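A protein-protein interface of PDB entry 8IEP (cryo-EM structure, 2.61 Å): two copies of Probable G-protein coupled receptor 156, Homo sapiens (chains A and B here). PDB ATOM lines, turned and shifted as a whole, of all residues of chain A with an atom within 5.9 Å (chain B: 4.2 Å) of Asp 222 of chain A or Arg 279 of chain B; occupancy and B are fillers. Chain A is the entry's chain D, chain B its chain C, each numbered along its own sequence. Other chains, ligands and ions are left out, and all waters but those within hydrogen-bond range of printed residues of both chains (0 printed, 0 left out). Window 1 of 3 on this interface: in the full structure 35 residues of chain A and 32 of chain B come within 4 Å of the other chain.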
ATOM      1  N   TYR A 220     -18.577  26.029  23.743  1.00  0.00           N
ATOM      2  CA  TYR A 220     -18.963  25.324  22.526  1.00  0.00           C
ATOM      3  C   TYR A 220     -19.583  26.322  21.560  1.00  0.00           C
ATOM      4  O   TYR A 220     -20.657  26.075  21.004  1.00  0.00           O
ATOM      5  CB  TYR A 220     -19.946  24.192  22.837  1.00  0.00           C
ATOM      6  CG  TYR A 220     -19.321  23.002  23.523  1.00  0.00           C
ATOM      7  CD1 TYR A 220     -19.291  22.914  24.906  1.00  0.00           C
ATOM      8  CD2 TYR A 220     -18.749  21.977  22.791  1.00  0.00           C
ATOM      9  CE1 TYR A 220     -18.721  21.831  25.540  1.00  0.00           C
ATOM     10  CE2 TYR A 220     -18.172  20.891  23.415  1.00  0.00           C
ATOM     11  CZ  TYR A 220     -18.162  20.824  24.791  1.00  0.00           C
ATOM     12  OH  TYR A 220     -17.589  19.742  25.417  1.00  0.00           O
ATOM     13  N   SER A 221     -18.911  27.458  21.370  1.00  0.00           N
ATOM     14  CA  SER A 221     -19.509  28.587  20.663  1.00  0.00           C
ATOM     15  C   SER A 221     -19.920  28.219  19.244  1.00  0.00           C
ATOM     16  O   SER A 221     -20.973  28.656  18.763  1.00  0.00           O
ATOM     17  CB  SER A 221     -18.526  29.755  20.639  1.00  0.00           C
ATOM     18  OG  SER A 221     -17.288  29.358  20.081  1.00  0.00           O
ATOM     19  N   ASP A 222     -19.100  27.431  18.549  1.00  0.00           N
ATOM     20  CA  ASP A 222     -19.419  27.082  17.170  1.00  0.00           C
ATOM     21  C   ASP A 222     -20.657  26.199  17.077  1.00  0.00           C
ATOM     22  O   ASP A 222     -21.335  26.212  16.050  1.00  0.00           O
ATOM     23  CB  ASP A 222     -18.216  26.413  16.509  1.00  0.00           C
ATOM     24  CG  ASP A 222     -17.082  27.382  16.257  1.00  0.00           C
ATOM     25  OD1 ASP A 222     -17.318  28.414  15.598  1.00  0.00           O
ATOM     26  OD2 ASP A 222     -15.959  27.124  16.733  1.00  0.00           O
ATOM     27  N   VAL A 223     -20.991  25.455  18.134  1.00  0.00           N
ATOM     28  CA  VAL A 223     -22.234  24.683  18.131  1.00  0.00           C
ATOM     29  C   VAL A 223     -23.432  25.620  18.047  1.00  0.00           C
ATOM     30  O   VAL A 223     -24.325  25.453  17.205  1.00  0.00           O
ATOM     31  CB  VAL A 223     -22.314  23.783  19.378  1.00  0.00           C
ATOM     32  CG1 VAL A 223     -23.640  23.034  19.417  1.00  0.00           C
ATOM     33  CG2 VAL A 223     -21.139  22.821  19.406  1.00  0.00           C
ATOM     34  N   TRP A 224     -23.449  26.642  18.904  1.00  0.00           N
ATOM     35  CA  TRP A 224     -24.571  27.571  18.919  1.00  0.00           C
ATOM     36  C   TRP A 224     -24.587  28.418  17.654  1.00  0.00           C
ATOM     37  O   TRP A 224     -25.658  28.753  17.134  1.00  0.00           O
ATOM     38  CB  TRP A 224     -24.506  28.441  20.175  1.00  0.00           C
ATOM     39  CG  TRP A 224     -24.299  27.656  21.431  1.00  0.00           C
ATOM     40  CD1 TRP A 224     -23.165  27.610  22.180  1.00  0.00           C
ATOM     41  CD2 TRP A 224     -25.255  26.819  22.094  1.00  0.00           C
ATOM     42  NE1 TRP A 224     -23.346  26.787  23.260  1.00  0.00           N
ATOM     43  CE2 TRP A 224     -24.622  26.291  23.233  1.00  0.00           C
ATOM     44  CE3 TRP A 224     -26.580  26.464  21.832  1.00  0.00           C
ATOM     45  CZ2 TRP A 224     -25.265  25.427  24.109  1.00  0.00           C
ATOM     46  CZ3 TRP A 224     -27.219  25.604  22.706  1.00  0.00           C
ATOM     47  CH2 TRP A 224     -26.560  25.095  23.831  1.00  0.00           C
ATOM     48  N   ILE A 225     -23.404  28.754  17.136  1.00  0.00           N
ATOM     49  CA  ILE A 225     -23.303  29.454  15.859  1.00  0.00           C
ATOM     50  C   ILE A 225     -23.921  28.630  14.741  1.00  0.00           C
ATOM     51  O   ILE A 225     -24.809  29.093  14.016  1.00  0.00           O
ATOM     52  CB  ILE A 225     -21.832  29.793  15.558  1.00  0.00           C
ATOM     53  CG1 ILE A 225     -21.377  30.928  16.482  1.00  0.00           C
ATOM     54  CG2 ILE A 225     -21.573  30.073  14.067  1.00  0.00           C
ATOM     55  CD1 ILE A 225     -19.909  30.936  16.746  1.00  0.00           C
ATOM     56  N   ALA A 226     -23.471  27.389  14.591  1.00  0.00           N
ATOM     57  CA  ALA A 226     -24.013  26.563  13.529  1.00  0.00           C
ATOM     58  C   ALA A 226     -25.516  26.404  13.686  1.00  0.00           C
ATOM     59  O   ALA A 226     -26.245  26.449  12.698  1.00  0.00           O
ATOM     60  CB  ALA A 226     -23.325  25.205  13.508  1.00  0.00           C
ATOM     61  N   LEU A 227     -26.002  26.288  14.921  1.00  0.00           N
ATOM     62  CA  LEU A 227     -27.438  26.130  15.133  1.00  0.00           C
ATOM     63  C   LEU A 227     -28.222  27.369  14.698  1.00  0.00           C
ATOM     64  O   LEU A 227     -29.246  27.254  14.013  1.00  0.00           O
ATOM     65  CB  LEU A 227     -27.712  25.802  16.600  1.00  0.00           C
ATOM     66  CG  LEU A 227     -27.823  24.314  16.950  1.00  0.00           C
ATOM     67  CD1 LEU A 227     -27.900  24.142  18.456  1.00  0.00           C
ATOM     68  CD2 LEU A 227     -29.030  23.662  16.290  1.00  0.00           C
ATOM     69  N   PHE A 275     -18.702  37.407  11.086  1.00  0.00           N
ATOM     70  CA  PHE A 275     -18.178  36.236  11.781  1.00  0.00           C
ATOM     71  C   PHE A 275     -16.660  36.164  11.660  1.00  0.00           C
ATOM     72  O   PHE A 275     -15.942  36.066  12.665  1.00  0.00           O
ATOM     73  CB  PHE A 275     -18.836  34.981  11.200  1.00  0.00           C
ATOM     74  CG  PHE A 275     -18.323  33.688  11.771  1.00  0.00           C
ATOM     75  CD1 PHE A 275     -18.409  33.424  13.126  1.00  0.00           C
ATOM     76  CD2 PHE A 275     -17.766  32.729  10.943  1.00  0.00           C
ATOM     77  CE1 PHE A 275     -17.941  32.230  13.642  1.00  0.00           C
ATOM     78  CE2 PHE A 275     -17.298  31.539  11.456  1.00  0.00           C
ATOM     79  CZ  PHE A 275     -17.387  31.288  12.805  1.00  0.00           C
ATOM     80  N   ARG A 279     -13.780  36.903  14.531  1.00  0.00           N
ATOM     81  CA  ARG A 279     -12.937  35.800  14.979  1.00  0.00           C
ATOM     82  C   ARG A 279     -11.455  36.125  14.835  1.00  0.00           C
ATOM     83  O   ARG A 279     -10.667  35.844  15.746  1.00  0.00           O
ATOM     84  CB  ARG A 279     -13.286  34.533  14.204  1.00  0.00           C
ATOM     85  CG  ARG A 279     -12.607  33.283  14.728  1.00  0.00           C
ATOM     86  CD  ARG A 279     -13.042  32.066  13.948  1.00  0.00           C
ATOM     87  NE  ARG A 279     -14.328  31.562  14.415  1.00  0.00           N
ATOM     88  CZ  ARG A 279     -14.498  30.718  15.425  1.00  0.00           C
ATOM     89  NH1 ARG A 279     -13.474  30.243  16.117  1.00  0.00           N
ATOM     90  NH2 ARG A 279     -15.729  30.339  15.751  1.00  0.00           N
ATOM     91  N   SER B 221      -8.599  28.796   8.949  1.00  0.00           N
ATOM     92  CA  SER B 221      -9.496  27.841   8.310  1.00  0.00           C
ATOM     93  C   SER B 221     -10.935  28.327   8.274  1.00  0.00           C
ATOM     94  O   SER B 221     -11.678  27.989   7.344  1.00  0.00           O
ATOM     95  CB  SER B 221      -9.429  26.498   9.037  1.00  0.00           C
ATOM     96  OG  SER B 221      -9.894  26.616  10.369  1.00  0.00           O
ATOM     97  N   ASP B 222     -11.342  29.123   9.262  1.00  0.00           N
ATOM     98  CA  ASP B 222     -12.703  29.632   9.283  1.00  0.00           C
ATOM     99  C   ASP B 222     -12.951  30.681   8.207  1.00  0.00           C
ATOM    100  O   ASP B 222     -14.093  30.834   7.777  1.00  0.00           O
ATOM    101  CB  ASP B 222     -13.030  30.186  10.668  1.00  0.00           C
ATOM    102  CG  ASP B 222     -13.038  29.113  11.728  1.00  0.00           C
ATOM    103  OD1 ASP B 222     -13.790  28.130  11.574  1.00  0.00           O
ATOM    104  OD2 ASP B 222     -12.283  29.242  12.713  1.00  0.00           O
ATOM    105  N   PHE B 275     -19.988  20.055   9.990  1.00  0.00           N
ATOM    106  CA  PHE B 275     -19.044  21.060  10.463  1.00  0.00           C
ATOM    107  C   PHE B 275     -18.899  20.996  11.977  1.00  0.00           C
ATOM    108  O   PHE B 275     -17.780  20.918  12.499  1.00  0.00           O
ATOM    109  CB  PHE B 275     -19.509  22.447  10.013  1.00  0.00           C
ATOM    110  CG  PHE B 275     -18.784  23.589  10.673  1.00  0.00           C
ATOM    111  CD1 PHE B 275     -17.436  23.801  10.449  1.00  0.00           C
ATOM    112  CD2 PHE B 275     -19.458  24.459  11.514  1.00  0.00           C
ATOM    113  CE1 PHE B 275     -16.776  24.854  11.053  1.00  0.00           C
ATOM    114  CE2 PHE B 275     -18.801  25.509  12.117  1.00  0.00           C
ATOM    115  CZ  PHE B 275     -17.461  25.707  11.886  1.00  0.00           C
ATOM    116  N   VAL B 276     -20.025  20.979  12.700  1.00  0.00           N
ATOM    117  CA  VAL B 276     -19.960  20.940  14.160  1.00  0.00           C
ATOM    118  C   VAL B 276     -19.311  19.642  14.636  1.00  0.00           C
ATOM    119  O   VAL B 276     -18.444  19.649  15.521  1.00  0.00           O
ATOM    120  CB  VAL B 276     -21.366  21.122  14.760  1.00  0.00           C
ATOM    121  CG1 VAL B 276     -21.385  20.748  16.237  1.00  0.00           C
ATOM    122  CG2 VAL B 276     -21.827  22.543  14.577  1.00  0.00           C
ATOM    123  N   VAL B 277     -19.722  18.512  14.059  1.00  0.00           N
ATOM    124  CA  VAL B 277     -19.232  17.215  14.512  1.00  0.00           C
ATOM    125  C   VAL B 277     -17.734  17.088  14.267  1.00  0.00           C
ATOM    126  O   VAL B 277     -16.993  16.600  15.127  1.00  0.00           O
ATOM    127  CB  VAL B 277     -20.027  16.089  13.824  1.00  0.00           C
ATOM    128  CG1 VAL B 277     -19.328  14.748  13.980  1.00  0.00           C
ATOM    129  CG2 VAL B 277     -21.432  16.018  14.397  1.00  0.00           C
ATOM    130  N   THR B 278     -17.261  17.513  13.095  1.00  0.00           N
ATOM    131  CA  THR B 278     -15.830  17.485  12.829  1.00  0.00           C
ATOM    132  C   THR B 278     -15.079  18.412  13.774  1.00  0.00           C
ATOM    133  O   THR B 278     -13.991  18.071  14.249  1.00  0.00           O
ATOM    134  CB  THR B 278     -15.561  17.869  11.376  1.00  0.00           C
ATOM    135  OG1 THR B 278     -16.364  17.059  10.510  1.00  0.00           O
ATOM    136  CG2 THR B 278     -14.096  17.676  11.028  1.00  0.00           C
ATOM    137  N   ARG B 279     -15.640  19.591  14.058  1.00  0.00           N
ATOM    138  CA  ARG B 279     -14.935  20.540  14.911  1.00  0.00           C
ATOM    139  C   ARG B 279     -14.772  20.012  16.330  1.00  0.00           C
ATOM    140  O   ARG B 279     -13.682  20.108  16.906  1.00  0.00           O
ATOM    141  CB  ARG B 279     -15.669  21.879  14.925  1.00  0.00           C
ATOM    142  CG  ARG B 279     -14.951  22.950  15.726  1.00  0.00           C
ATOM    143  CD  ARG B 279     -15.093  24.320  15.098  1.00  0.00           C
ATOM    144  NE  ARG B 279     -14.028  24.585  14.139  1.00  0.00           N
ATOM    145  CZ  ARG B 279     -13.896  25.707  13.444  1.00  0.00           C
ATOM    146  NH1 ARG B 279     -14.748  26.712  13.578  1.00  0.00           N
ATOM    147  NH2 ARG B 279     -12.885  25.825  12.591  1.00  0.00           N
ATOM    148  N   TYR B 280     -15.832  19.446  16.910  1.00  0.00           N
ATOM    149  CA  TYR B 280     -15.844  19.138  18.340  1.00  0.00           C
ATOM    150  C   TYR B 280     -15.725  17.662  18.674  1.00  0.00           C
ATOM    151  O   TYR B 280     -15.054  17.323  19.650  1.00  0.00           O
ATOM    152  CB  TYR B 280     -17.115  19.703  18.981  1.00  0.00           C
ATOM    153  CG  TYR B 280     -17.044  21.199  19.156  1.00  0.00           C
ATOM    154  CD1 TYR B 280     -16.130  21.767  20.028  1.00  0.00           C
ATOM    155  CD2 TYR B 280     -17.864  22.042  18.429  1.00  0.00           C
ATOM    156  CE1 TYR B 280     -16.045  23.124  20.183  1.00  0.00           C
ATOM    157  CE2 TYR B 280     -17.784  23.401  18.577  1.00  0.00           C
ATOM    158  CZ  TYR B 280     -16.871  23.940  19.457  1.00  0.00           C
ATOM    159  OH  TYR B 280     -16.772  25.300  19.630  1.00  0.00           O
ATOM    160  N   LEU B 281     -16.347  16.769  17.913  1.00  0.00           N
ATOM    161  CA  LEU B 281     -16.244  15.337  18.193  1.00  0.00           C
ATOM    162  C   LEU B 281     -15.098  14.701  17.414  1.00  0.00           C
ATOM    163  O   LEU B 281     -15.261  13.679  16.753  1.00  0.00           O
ATOM    164  CB  LEU B 281     -17.569  14.654  17.881  1.00  0.00           C
ATOM    165  CG  LEU B 281     -18.740  15.059  18.779  1.00  0.00           C
ATOM    166  CD1 LEU B 281     -20.045  14.527  18.223  1.00  0.00           C
ATOM    167  CD2 LEU B 281     -18.535  14.575  20.205  1.00  0.00           C
ATOM    168  N   HIS B 282     -13.912  15.302  17.507  1.00  0.00           N
ATOM    169  CA  HIS B 282     -12.735  14.768  16.835  1.00  0.00           C
ATOM    170  C   HIS B 282     -12.151  13.552  17.542  1.00  0.00           C
ATOM    171  O   HIS B 282     -11.375  12.815  16.926  1.00  0.00           O
ATOM    172  CB  HIS B 282     -11.659  15.851  16.707  1.00  0.00           C
ATOM    173  CG  HIS B 282     -11.133  16.344  18.019  1.00  0.00           C
ATOM    174  ND1 HIS B 282     -11.755  17.337  18.745  1.00  0.00           N
ATOM    175  CD2 HIS B 282     -10.043  15.982  18.736  1.00  0.00           C
ATOM    176  CE1 HIS B 282     -11.072  17.565  19.852  1.00  0.00           C
ATOM    177  NE2 HIS B 282     -10.028  16.754  19.870  1.00  0.00           N
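The backbone NH (N) of Asp 222 of chain A sits at hydrogen-bond distance from the side-chain hydroxyl (OH) of Tyr 280 of chain B (3.3 Å). The guanidinium group (NH1) of Arg 279 of chain B lies within salt-bridge range of the side-chain carboxylate (OD2) of Asp 222 of chain A, at 3.4 Å. OD2 of Asp 222 of chain B is in salt-bridge range of NE of Arg 279 of chain A (3.5 Å).
Tyr 220 of chain A touches Tyr 280 of chain B. OH of Tyr 280 of chain B touches N of Ser 221 of chain A (3.5 Å). Val 276 of chain B touches Asp 222 of chain A. Val 223 of chain A touches Val 276 of chain B. CG2 of Val 223 of chain A touches CE2 of Tyr 280 of chain B, at 3.5 Å. Val 276 of chain B touches Ala 226 of chain A (CG2 to CB, 3.2 Å).
Trp 224 of chain A touches none of the printed residues of chain B. Of the printed residues of chain B, Ala 226 of chain A touches Val 276. Of the printed residues of chain B, Arg 279 of chain A touches Asp 222. Of the printed residues of chain A, Arg 279 of chain B touches Asp 222 (3.4 Å).
Asp 222 of chain A touches Arg 279 of chain B, and with the chains exchanged Arg 279 of chain A touches Asp 222 of chain B. Of the 9 pairs that touch across the chains among the printed residues, 2 have their exchanged pair printed and touching as well.
Of the 10 printed residues of chain A, 6 touch a printed residue of chain B. Printed residues of chain A that touch a printed residue of chain B: Tyr 220, Ser 221, Asp 222, Val 223, Ala 226 and Arg 279. Printed residues of chain B that touch a printed residue of chain A: Asp 222, Val 276, Arg 279 and Tyr 280. Hydrophobic or aromatic side chains of chain B that line the printed part of chain A: Val 276 and Tyr 280. Among the printed residues, 9 pairs touch across the chains. Among the printed residues, Asp or Glu carboxylates within 4 Å of a Lys or Arg side-chain nitrogen of the other chain: Asp 222 of chain A with Arg 279 of chain B (3.4 Å) and Arg 279 of chain A with Asp 222 of chain B (3.5 Å).
The guanidinium group of Arg 279 of chain B lies within salt-bridge range of the side-chain carboxylate of Asp 222 of chain B, at 2.6 Å. OD1 of Asp 222 of chain A is in salt-bridge range of NH2 of Arg 279 of chain A. The backbone carbonyl oxygen (O) of Tyr 280 of chain B is in hydrogen-bond range of a ring nitrogen (ND1) of His 282 of chain B, 3.4 Å away.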
